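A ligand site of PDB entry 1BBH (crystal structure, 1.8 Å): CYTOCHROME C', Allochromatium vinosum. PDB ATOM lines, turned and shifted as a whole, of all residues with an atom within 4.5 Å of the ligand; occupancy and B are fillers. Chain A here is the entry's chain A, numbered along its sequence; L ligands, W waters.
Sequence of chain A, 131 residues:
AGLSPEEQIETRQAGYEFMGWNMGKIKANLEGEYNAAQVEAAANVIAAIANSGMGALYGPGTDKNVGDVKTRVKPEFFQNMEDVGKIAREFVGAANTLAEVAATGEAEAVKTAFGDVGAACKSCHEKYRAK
The side-chain sulfur (SG) of Cys 124 is covalently linked to a carbon (C25) of the ligand, 1.9 Å away.
NH1 of Arg 12 lies within salt-bridge range of O4 of the ligand (3.0 Å).
A ring nitrogen (NE2) of His 125 is bound to an iron atom (FE1) of the ligand (2.0 Å).
SG of Cys 121 is bonded to C18 of the ligand, at 1.9 Å.
The side-chain amide nitrogen (NE2) of Gln 13 lies within hydrogen-bond range of an oxygen (O3) of the ligand.
The backbone NH (N) of Arg 72 sits at hydrogen-bond distance from an oxygen (O3) of the ligand, at 2.8 Å.
The side-chain hydroxyl of Tyr 16 lies within hydrogen-bond range of the side-chain hydroxyl of Tyr 58, at 2.8 Å.
The guanidinium group (NH2) of Arg 129 lies close to a ring nitrogen (ND1) of His 125, 3.3 Å away.
Tyr 16 touches the ligand.
CA of Gly 20 touches C17 of the ligand, at 3.9 Å.
CG of Met 23 touches C17 of the ligand (3.97 Å).
Tyr 58 touches the ligand (OH to C31, 3.4 Å).
Thr 71 touches the ligand.
Val 73 touches the ligand (CG2 to C31, 3.7 Å).
CE1 of Phe 91 touches C19 of the ligand, at 3.5 Å.
Val 117 touches the ligand.
Tyr 128 touches the ligand (O to C31, 3.9 Å).
NH2 of Arg 129 touches C5 of the ligand (3.6 Å).
Hydrophobic or aromatic side chains that line the ligand: Tyr 16, Met 23, Val 73, Phe 91, Val 117 and His 125.
The nearest printed residue that does not touch the ligand is Glu 17 (4.04 Å).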
ATOM      1  N   ILE A   9       3.591  21.755  18.127  1.00  0.00           N
ATOM      2  CA  ILE A   9       3.211  21.564  16.736  1.00  0.00           C
ATOM      3  C   ILE A   9       1.698  21.801  16.540  1.00  0.00           C
ATOM      4  O   ILE A   9       1.295  22.557  15.649  1.00  0.00           O
ATOM      5  CB  ILE A   9       3.639  20.134  16.289  1.00  0.00           C
ATOM      6  CG1 ILE A   9       5.207  20.068  16.255  1.00  0.00           C
ATOM      7  CG2 ILE A   9       2.978  19.785  14.918  1.00  0.00           C
ATOM      8  CD1 ILE A   9       5.596  18.577  16.141  1.00  0.00           C
ATOM      9  N   ARG A  12       0.922  25.724  16.804  1.00  0.00           N
ATOM     10  CA  ARG A  12       1.289  26.647  15.712  1.00  0.00           C
ATOM     11  C   ARG A  12       0.325  26.323  14.571  1.00  0.00           C
ATOM     12  O   ARG A  12      -0.151  27.196  13.866  1.00  0.00           O
ATOM     13  CB  ARG A  12       2.832  26.423  15.265  1.00  0.00           C
ATOM     14  CG  ARG A  12       3.031  24.962  14.857  1.00  0.00           C
ATOM     15  CD  ARG A  12       4.219  24.582  14.052  1.00  0.00           C
ATOM     16  NE  ARG A  12       5.293  24.255  14.901  1.00  0.00           N
ATOM     17  CZ  ARG A  12       6.275  23.377  14.655  1.00  0.00           C
ATOM     18  NH1 ARG A  12       6.459  22.534  13.616  1.00  0.00           N
ATOM     19  NH2 ARG A  12       7.155  23.371  15.626  1.00  0.00           N
ATOM     20  N   GLN A  13      -0.045  25.062  14.405  1.00  0.00           N
ATOM     21  CA  GLN A  13      -0.952  24.696  13.346  1.00  0.00           C
ATOM     22  C   GLN A  13      -2.315  25.349  13.637  1.00  0.00           C
ATOM     23  O   GLN A  13      -2.920  25.888  12.724  1.00  0.00           O
ATOM     24  CB  GLN A  13      -1.073  23.190  13.281  1.00  0.00           C
ATOM     25  CG  GLN A  13       0.195  22.537  12.640  1.00  0.00           C
ATOM     26  CD  GLN A  13       0.185  21.033  12.688  1.00  0.00           C
ATOM     27  OE1 GLN A  13      -0.633  20.437  13.383  1.00  0.00           O
ATOM     28  NE2 GLN A  13       1.051  20.272  12.049  1.00  0.00           N
ATOM     29  N   TYR A  16      -2.050  29.071  12.604  1.00  0.00           N
ATOM     30  CA  TYR A  16      -2.073  29.207  11.155  1.00  0.00           C
ATOM     31  C   TYR A  16      -3.457  28.963  10.553  1.00  0.00           C
ATOM     32  O   TYR A  16      -3.903  29.682   9.662  1.00  0.00           O
ATOM     33  CB  TYR A  16      -1.128  28.213  10.484  1.00  0.00           C
ATOM     34  CG  TYR A  16       0.352  28.560  10.697  1.00  0.00           C
ATOM     35  CD1 TYR A  16       0.776  29.883  10.513  1.00  0.00           C
ATOM     36  CD2 TYR A  16       1.255  27.571  11.110  1.00  0.00           C
ATOM     37  CE1 TYR A  16       2.112  30.254  10.766  1.00  0.00           C
ATOM     38  CE2 TYR A  16       2.587  27.934  11.352  1.00  0.00           C
ATOM     39  CZ  TYR A  16       2.969  29.249  11.171  1.00  0.00           C
ATOM     40  OH  TYR A  16       4.278  29.488  11.448  1.00  0.00           O
ATOM     41  N   GLU A  17      -4.105  27.947  11.026  1.00  0.00           N
ATOM     42  CA  GLU A  17      -5.452  27.595  10.579  1.00  0.00           C
ATOM     43  C   GLU A  17      -6.476  28.691  10.875  1.00  0.00           C
ATOM     44  O   GLU A  17      -7.254  29.086   9.990  1.00  0.00           O
ATOM     45  CB  GLU A  17      -5.825  26.351  11.263  1.00  0.00           C
ATOM     46  CG  GLU A  17      -7.161  25.795  10.735  1.00  0.00           C
ATOM     47  CD  GLU A  17      -8.279  26.156  11.695  1.00  0.00           C
ATOM     48  OE1 GLU A  17      -8.689  27.347  11.801  1.00  0.00           O
ATOM     49  OE2 GLU A  17      -8.863  25.207  12.261  1.00  0.00           O
ATOM     50  N   MET A  19      -5.774  31.887  11.235  1.00  0.00           N
ATOM     51  CA  MET A  19      -5.502  32.972  10.289  1.00  0.00           C
ATOM     52  C   MET A  19      -6.084  32.678   8.931  1.00  0.00           C
ATOM     53  O   MET A  19      -6.649  33.588   8.303  1.00  0.00           O
ATOM     54  CB  MET A  19      -3.984  33.248  10.079  1.00  0.00           C
ATOM     55  CG  MET A  19      -3.397  33.905  11.330  1.00  0.00           C
ATOM     56  SD  MET A  19      -1.785  34.713  10.982  1.00  0.00           S
ATOM     57  CE  MET A  19      -0.791  33.261  10.845  1.00  0.00           C
ATOM     58  N   GLY A  20      -6.021  31.451   8.479  1.00  0.00           N
ATOM     59  CA  GLY A  20      -6.596  31.066   7.214  1.00  0.00           C
ATOM     60  C   GLY A  20      -8.118  31.369   7.176  1.00  0.00           C
ATOM     61  O   GLY A  20      -8.597  31.947   6.195  1.00  0.00           O
ATOM     62  N   MET A  23      -8.508  34.959   6.723  1.00  0.00           N
ATOM     63  CA  MET A  23      -8.112  35.380   5.404  1.00  0.00           C
ATOM     64  C   MET A  23      -9.277  35.140   4.445  1.00  0.00           C
ATOM     65  O   MET A  23      -9.685  36.024   3.688  1.00  0.00           O
ATOM     66  CB  MET A  23      -6.876  34.599   4.960  1.00  0.00           C
ATOM     67  CG  MET A  23      -5.525  35.084   5.474  1.00  0.00           C
ATOM     68  SD  MET A  23      -5.064  36.767   5.089  1.00  0.00           S
ATOM     69  CE  MET A  23      -4.266  36.402   3.545  1.00  0.00           C
ATOM     70  N   ILE A  46      -5.473  38.754  12.246  1.00  0.00           N
ATOM     71  CA  ILE A  46      -4.231  38.358  11.570  1.00  0.00           C
ATOM     72  C   ILE A  46      -3.025  39.139  12.135  1.00  0.00           C
ATOM     73  O   ILE A  46      -1.941  38.547  12.398  1.00  0.00           O
ATOM     74  CB  ILE A  46      -4.440  38.564  10.032  1.00  0.00           C
ATOM     75  CG1 ILE A  46      -5.466  37.499   9.490  1.00  0.00           C
ATOM     76  CG2 ILE A  46      -3.091  38.370   9.281  1.00  0.00           C
ATOM     77  CD1 ILE A  46      -6.136  38.056   8.219  1.00  0.00           C
ATOM     78  N   TYR A  58       8.527  26.898  17.733  1.00  0.00           N
ATOM     79  CA  TYR A  58       9.439  26.057  16.954  1.00  0.00           C
ATOM     80  C   TYR A  58      10.650  25.709  17.839  1.00  0.00           C
ATOM     81  O   TYR A  58      11.799  26.073  17.559  1.00  0.00           O
ATOM     82  CB  TYR A  58       9.868  26.841  15.709  1.00  0.00           C
ATOM     83  CG  TYR A  58       8.772  26.919  14.648  1.00  0.00           C
ATOM     84  CD1 TYR A  58       8.602  25.889  13.766  1.00  0.00           C
ATOM     85  CD2 TYR A  58       7.952  28.031  14.572  1.00  0.00           C
ATOM     86  CE1 TYR A  58       7.627  25.932  12.788  1.00  0.00           C
ATOM     87  CE2 TYR A  58       6.962  28.102  13.613  1.00  0.00           C
ATOM     88  CZ  TYR A  58       6.811  27.052  12.723  1.00  0.00           C
ATOM     89  OH  TYR A  58       5.827  27.166  11.745  1.00  0.00           O
ATOM     90  N   THR A  71       3.996  17.003  11.449  1.00  0.00           N
ATOM     91  CA  THR A  71       4.460  18.337  11.127  1.00  0.00           C
ATOM     92  C   THR A  71       4.584  18.389   9.620  1.00  0.00           C
ATOM     93  O   THR A  71       5.059  17.435   9.023  1.00  0.00           O
ATOM     94  CB  THR A  71       5.929  18.776  11.428  1.00  0.00           C
ATOM     95  OG1 THR A  71       6.753  17.860  12.172  1.00  0.00           O
ATOM     96  CG2 THR A  71       5.736  20.114  11.957  1.00  0.00           C
ATOM     97  N   ARG A  72       4.404  19.546   9.022  1.00  0.00           N
ATOM     98  CA  ARG A  72       4.771  19.734   7.632  1.00  0.00           C
ATOM     99  C   ARG A  72       5.956  20.685   7.610  1.00  0.00           C
ATOM    100  O   ARG A  72       6.279  21.217   6.540  1.00  0.00           O
ATOM    101  CB  ARG A  72       3.580  20.333   6.854  1.00  0.00           C
ATOM    102  CG  ARG A  72       2.453  19.285   6.803  1.00  0.00           C
ATOM    103  CD  ARG A  72       1.786  19.236   5.459  1.00  0.00           C
ATOM    104  NE  ARG A  72       1.110  20.471   5.170  1.00  0.00           N
ATOM    105  CZ  ARG A  72       0.897  20.880   3.922  1.00  0.00           C
ATOM    106  NH1 ARG A  72       1.285  20.223   2.817  1.00  0.00           N
ATOM    107  NH2 ARG A  72       0.275  22.014   3.805  1.00  0.00           N
ATOM    108  N   VAL A  73       6.613  21.042   8.708  1.00  0.00           N
ATOM    109  CA  VAL A  73       7.727  21.978   8.570  1.00  0.00           C
ATOM    110  C   VAL A  73       8.912  21.255   7.874  1.00  0.00           C
ATOM    111  O   VAL A  73       9.106  20.050   8.038  1.00  0.00           O
ATOM    112  CB  VAL A  73       8.097  22.543   9.967  1.00  0.00           C
ATOM    113  CG1 VAL A  73       8.778  21.553  10.918  1.00  0.00           C
ATOM    114  CG2 VAL A  73       8.935  23.779   9.701  1.00  0.00           C
ATOM    115  N   ILE A  87      11.506  36.910   6.665  1.00  0.00           N
ATOM    116  CA  ILE A  87      10.180  36.702   6.079  1.00  0.00           C
ATOM    117  C   ILE A  87       9.140  36.983   7.184  1.00  0.00           C
ATOM    118  O   ILE A  87       8.095  37.594   6.910  1.00  0.00           O
ATOM    119  CB  ILE A  87      10.011  35.241   5.580  1.00  0.00           C
ATOM    120  CG1 ILE A  87      11.029  34.910   4.477  1.00  0.00           C
ATOM    121  CG2 ILE A  87       8.574  35.082   5.069  1.00  0.00           C
ATOM    122  CD1 ILE A  87      11.027  33.444   3.944  1.00  0.00           C
ATOM    123  N   ALA A  88       9.449  36.599   8.435  1.00  0.00           N
ATOM    124  CA  ALA A  88       8.563  36.799   9.564  1.00  0.00           C
ATOM    125  C   ALA A  88       8.392  38.296   9.798  1.00  0.00           C
ATOM    126  O   ALA A  88       7.268  38.800  10.025  1.00  0.00           O
ATOM    127  CB  ALA A  88       9.156  36.098  10.802  1.00  0.00           C
ATOM    128  N   PHE A  91       6.137  39.679   7.111  1.00  0.00           N
ATOM    129  CA  PHE A  91       4.768  39.293   7.429  1.00  0.00           C
ATOM    130  C   PHE A  91       4.215  40.168   8.561  1.00  0.00           C
ATOM    131  O   PHE A  91       3.077  40.635   8.364  1.00  0.00           O
ATOM    132  CB  PHE A  91       4.761  37.789   7.772  1.00  0.00           C
ATOM    133  CG  PHE A  91       3.401  37.286   8.253  1.00  0.00           C
ATOM    134  CD1 PHE A  91       2.270  37.486   7.493  1.00  0.00           C
ATOM    135  CD2 PHE A  91       3.315  36.635   9.475  1.00  0.00           C
ATOM    136  CE1 PHE A  91       1.050  37.045   7.979  1.00  0.00           C
ATOM    137  CE2 PHE A  91       2.089  36.196   9.941  1.00  0.00           C
ATOM    138  CZ  PHE A  91       0.958  36.407   9.183  1.00  0.00           C
ATOM    139  N   VAL A 117      -0.438  40.615   2.196  1.00  0.00           N
ATOM    140  CA  VAL A 117      -0.364  39.657   3.287  1.00  0.00           C
ATOM    141  C   VAL A 117      -0.354  38.267   2.685  1.00  0.00           C
ATOM    142  O   VAL A 117       0.433  37.414   3.120  1.00  0.00           O
ATOM    143  CB  VAL A 117      -1.557  39.797   4.288  1.00  0.00           C
ATOM    144  CG1 VAL A 117      -1.574  38.645   5.247  1.00  0.00           C
ATOM    145  CG2 VAL A 117      -1.387  41.009   5.159  1.00  0.00           C
ATOM    146  N   ALA A 120       3.055  37.163   1.606  1.00  0.00           N
ATOM    147  CA  ALA A 120       3.942  36.796   2.660  1.00  0.00           C
ATOM    148  C   ALA A 120       3.581  35.417   3.165  1.00  0.00           C
ATOM    149  O   ALA A 120       4.508  34.634   3.415  1.00  0.00           O
ATOM    150  CB  ALA A 120       3.833  37.841   3.751  1.00  0.00           C
ATOM    151  N   CYS A 121       2.299  34.990   3.238  1.00  0.00           N
ATOM    152  CA  CYS A 121       2.014  33.623   3.689  1.00  0.00           C
ATOM    153  C   CYS A 121       2.665  32.647   2.703  1.00  0.00           C
ATOM    154  O   CYS A 121       3.279  31.639   3.071  1.00  0.00           O
ATOM    155  CB  CYS A 121       0.520  33.306   3.685  1.00  0.00           C
ATOM    156  SG  CYS A 121      -0.451  34.574   4.545  1.00  0.00           S
ATOM    157  N   CYS A 124       6.735  32.201   2.714  1.00  0.00           N
ATOM    158  CA  CYS A 124       7.249  31.289   3.698  1.00  0.00           C
ATOM    159  C   CYS A 124       6.863  29.851   3.400  1.00  0.00           C
ATOM    160  O   CYS A 124       7.669  28.941   3.579  1.00  0.00           O
ATOM    161  CB  CYS A 124       6.741  31.685   5.066  1.00  0.00           C
ATOM    162  SG  CYS A 124       7.366  30.668   6.424  1.00  0.00           S
ATOM    163  N   HIS A 125       5.662  29.569   2.881  1.00  0.00           N
ATOM    164  CA  HIS A 125       5.226  28.194   2.586  1.00  0.00           C
ATOM    165  C   HIS A 125       6.059  27.561   1.487  1.00  0.00           C
ATOM    166  O   HIS A 125       6.445  26.401   1.593  1.00  0.00           O
ATOM    167  CB  HIS A 125       3.742  28.104   2.119  1.00  0.00           C
ATOM    168  CG  HIS A 125       2.725  28.393   3.228  1.00  0.00           C
ATOM    169  ND1 HIS A 125       1.435  28.645   3.067  1.00  0.00           N
ATOM    170  CD2 HIS A 125       2.997  28.525   4.584  1.00  0.00           C
ATOM    171  CE1 HIS A 125       0.928  28.938   4.252  1.00  0.00           C
ATOM    172  NE2 HIS A 125       1.854  28.873   5.180  1.00  0.00           N
ATOM    173  N   TYR A 128       9.581  26.812   3.145  1.00  0.00           N
ATOM    174  CA  TYR A 128       9.686  26.066   4.410  1.00  0.00           C
ATOM    175  C   TYR A 128       8.564  25.136   4.783  1.00  0.00           C
ATOM    176  O   TYR A 128       8.581  24.619   5.924  1.00  0.00           O
ATOM    177  CB  TYR A 128       9.866  27.069   5.550  1.00  0.00           C
ATOM    178  CG  TYR A 128      11.107  27.900   5.389  1.00  0.00           C
ATOM    179  CD1 TYR A 128      12.323  27.226   5.388  1.00  0.00           C
ATOM    180  CD2 TYR A 128      11.031  29.270   5.217  1.00  0.00           C
ATOM    181  CE1 TYR A 128      13.493  27.962   5.208  1.00  0.00           C
ATOM    182  CE2 TYR A 128      12.173  30.010   5.015  1.00  0.00           C
ATOM    183  CZ  TYR A 128      13.391  29.326   5.022  1.00  0.00           C
ATOM    184  OH  TYR A 128      14.574  30.010   4.853  1.00  0.00           O
ATOM    185  N   ARG A 129       7.567  24.897   3.917  1.00  0.00           N
ATOM    186  CA  ARG A 129       6.544  23.968   4.333  1.00  0.00           C
ATOM    187  C   ARG A 129       6.569  22.904   3.277  1.00  0.00           C
ATOM    188  O   ARG A 129       6.600  23.194   2.073  1.00  0.00           O
ATOM    189  CB  ARG A 129       5.193  24.672   4.404  1.00  0.00           C
ATOM    190  CG  ARG A 129       4.159  23.714   4.915  1.00  0.00           C
ATOM    191  CD  ARG A 129       3.048  23.879   3.901  1.00  0.00           C
ATOM    192  NE  ARG A 129       2.006  24.756   4.283  1.00  0.00           N
ATOM    193  CZ  ARG A 129       1.012  25.212   3.508  1.00  0.00           C
ATOM    194  NH1 ARG A 129       0.921  25.250   2.176  1.00  0.00           N
ATOM    195  NH2 ARG A 129       0.076  25.858   4.135  1.00  0.00           N
HETATM  196 FE1  LIG L   1       1.544  29.066   7.158  1.00  0.00          FE
HETATM  197  C1  LIG L   1       1.145  25.833   8.007  1.00  0.00           C
HETATM  198  C2  LIG L   1      -1.748  29.387   6.739  1.00  0.00           C
HETATM  199  C3  LIG L   1       1.853  32.482   7.143  1.00  0.00           C
HETATM  200  C4  LIG L   1       4.867  28.816   7.860  1.00  0.00           C
HETATM  201  N1  LIG L   1      -0.032  27.780   7.331  1.00  0.00           N
HETATM  202  C5  LIG L   1      -0.013  26.507   7.672  1.00  0.00           C
HETATM  203  C6  LIG L   1      -1.308  25.972   7.620  1.00  0.00           C
HETATM  204  C7  LIG L   1      -2.130  27.032   7.253  1.00  0.00           C
HETATM  205  C8  LIG L   1      -1.301  28.117   7.099  1.00  0.00           C
HETATM  206  C9  LIG L   1      -3.642  27.011   7.015  1.00  0.00           C
HETATM  207  C10 LIG L   1      -1.750  24.552   7.883  1.00  0.00           C
HETATM  208  C11 LIG L   1      -1.981  24.306   9.369  1.00  0.00           C
HETATM  209  C12 LIG L   1      -2.508  22.908   9.662  1.00  0.00           C
HETATM  210  O1  LIG L   1      -3.729  22.776   9.772  1.00  0.00           O
HETATM  211  O2  LIG L   1      -1.762  21.947   9.791  1.00  0.00           O
HETATM  212  N2  LIG L   1       0.255  30.672   7.029  1.00  0.00           N
HETATM  213  C13 LIG L   1      -1.043  30.577   6.712  1.00  0.00           C
HETATM  214  C14 LIG L   1      -1.586  31.812   6.348  1.00  0.00           C
HETATM  215  C15 LIG L   1      -0.539  32.735   6.485  1.00  0.00           C
HETATM  216  C16 LIG L   1       0.561  31.976   6.903  1.00  0.00           C
HETATM  217  C17 LIG L   1      -3.017  32.033   5.859  1.00  0.00           C
HETATM  218  C18 LIG L   1      -0.518  34.146   6.349  1.00  0.00           C
HETATM  219  C19 LIG L   1      -1.624  35.028   6.826  1.00  0.00           C
HETATM  220  N3  LIG L   1       3.081  30.413   7.502  1.00  0.00           N
HETATM  221  C20 LIG L   1       3.021  31.741   7.446  1.00  0.00           C
HETATM  222  C21 LIG L   1       4.279  32.311   7.673  1.00  0.00           C
HETATM  223  C22 LIG L   1       5.195  31.268   7.811  1.00  0.00           C
HETATM  224  C23 LIG L   1       4.406  30.115   7.710  1.00  0.00           C
HETATM  225  C24 LIG L   1       4.485  33.815   7.614  1.00  0.00           C
HETATM  226  C25 LIG L   1       6.628  31.359   7.998  1.00  0.00           C
HETATM  227  C26 LIG L   1       7.403  32.619   8.338  1.00  0.00           C
HETATM  228  N4  LIG L   1       2.791  27.570   7.822  1.00  0.00           N
HETATM  229  C27 LIG L   1       4.134  27.640   7.961  1.00  0.00           C
HETATM  230  C28 LIG L   1       4.671  26.400   8.274  1.00  0.00           C
HETATM  231  C29 LIG L   1       3.587  25.553   8.307  1.00  0.00           C
HETATM  232  C30 LIG L   1       2.465  26.318   8.045  1.00  0.00           C
HETATM  233  C31 LIG L   1       6.129  25.985   8.573  1.00  0.00           C
HETATM  234  C32 LIG L   1       3.624  24.101   8.716  1.00  0.00           C
HETATM  235  C33 LIG L   1       3.475  24.017  10.248  1.00  0.00           C
HETATM  236  C34 LIG L   1       3.517  22.601  10.797  1.00  0.00           C
HETATM  237  O3  LIG L   1       3.025  21.641  10.209  1.00  0.00           O
HETATM  238  O4  LIG L   1       4.067  22.443  11.868  1.00  0.00           O
HETATM  239  O   HOH W   1       0.813  21.922   8.659  1.00  0.00           O
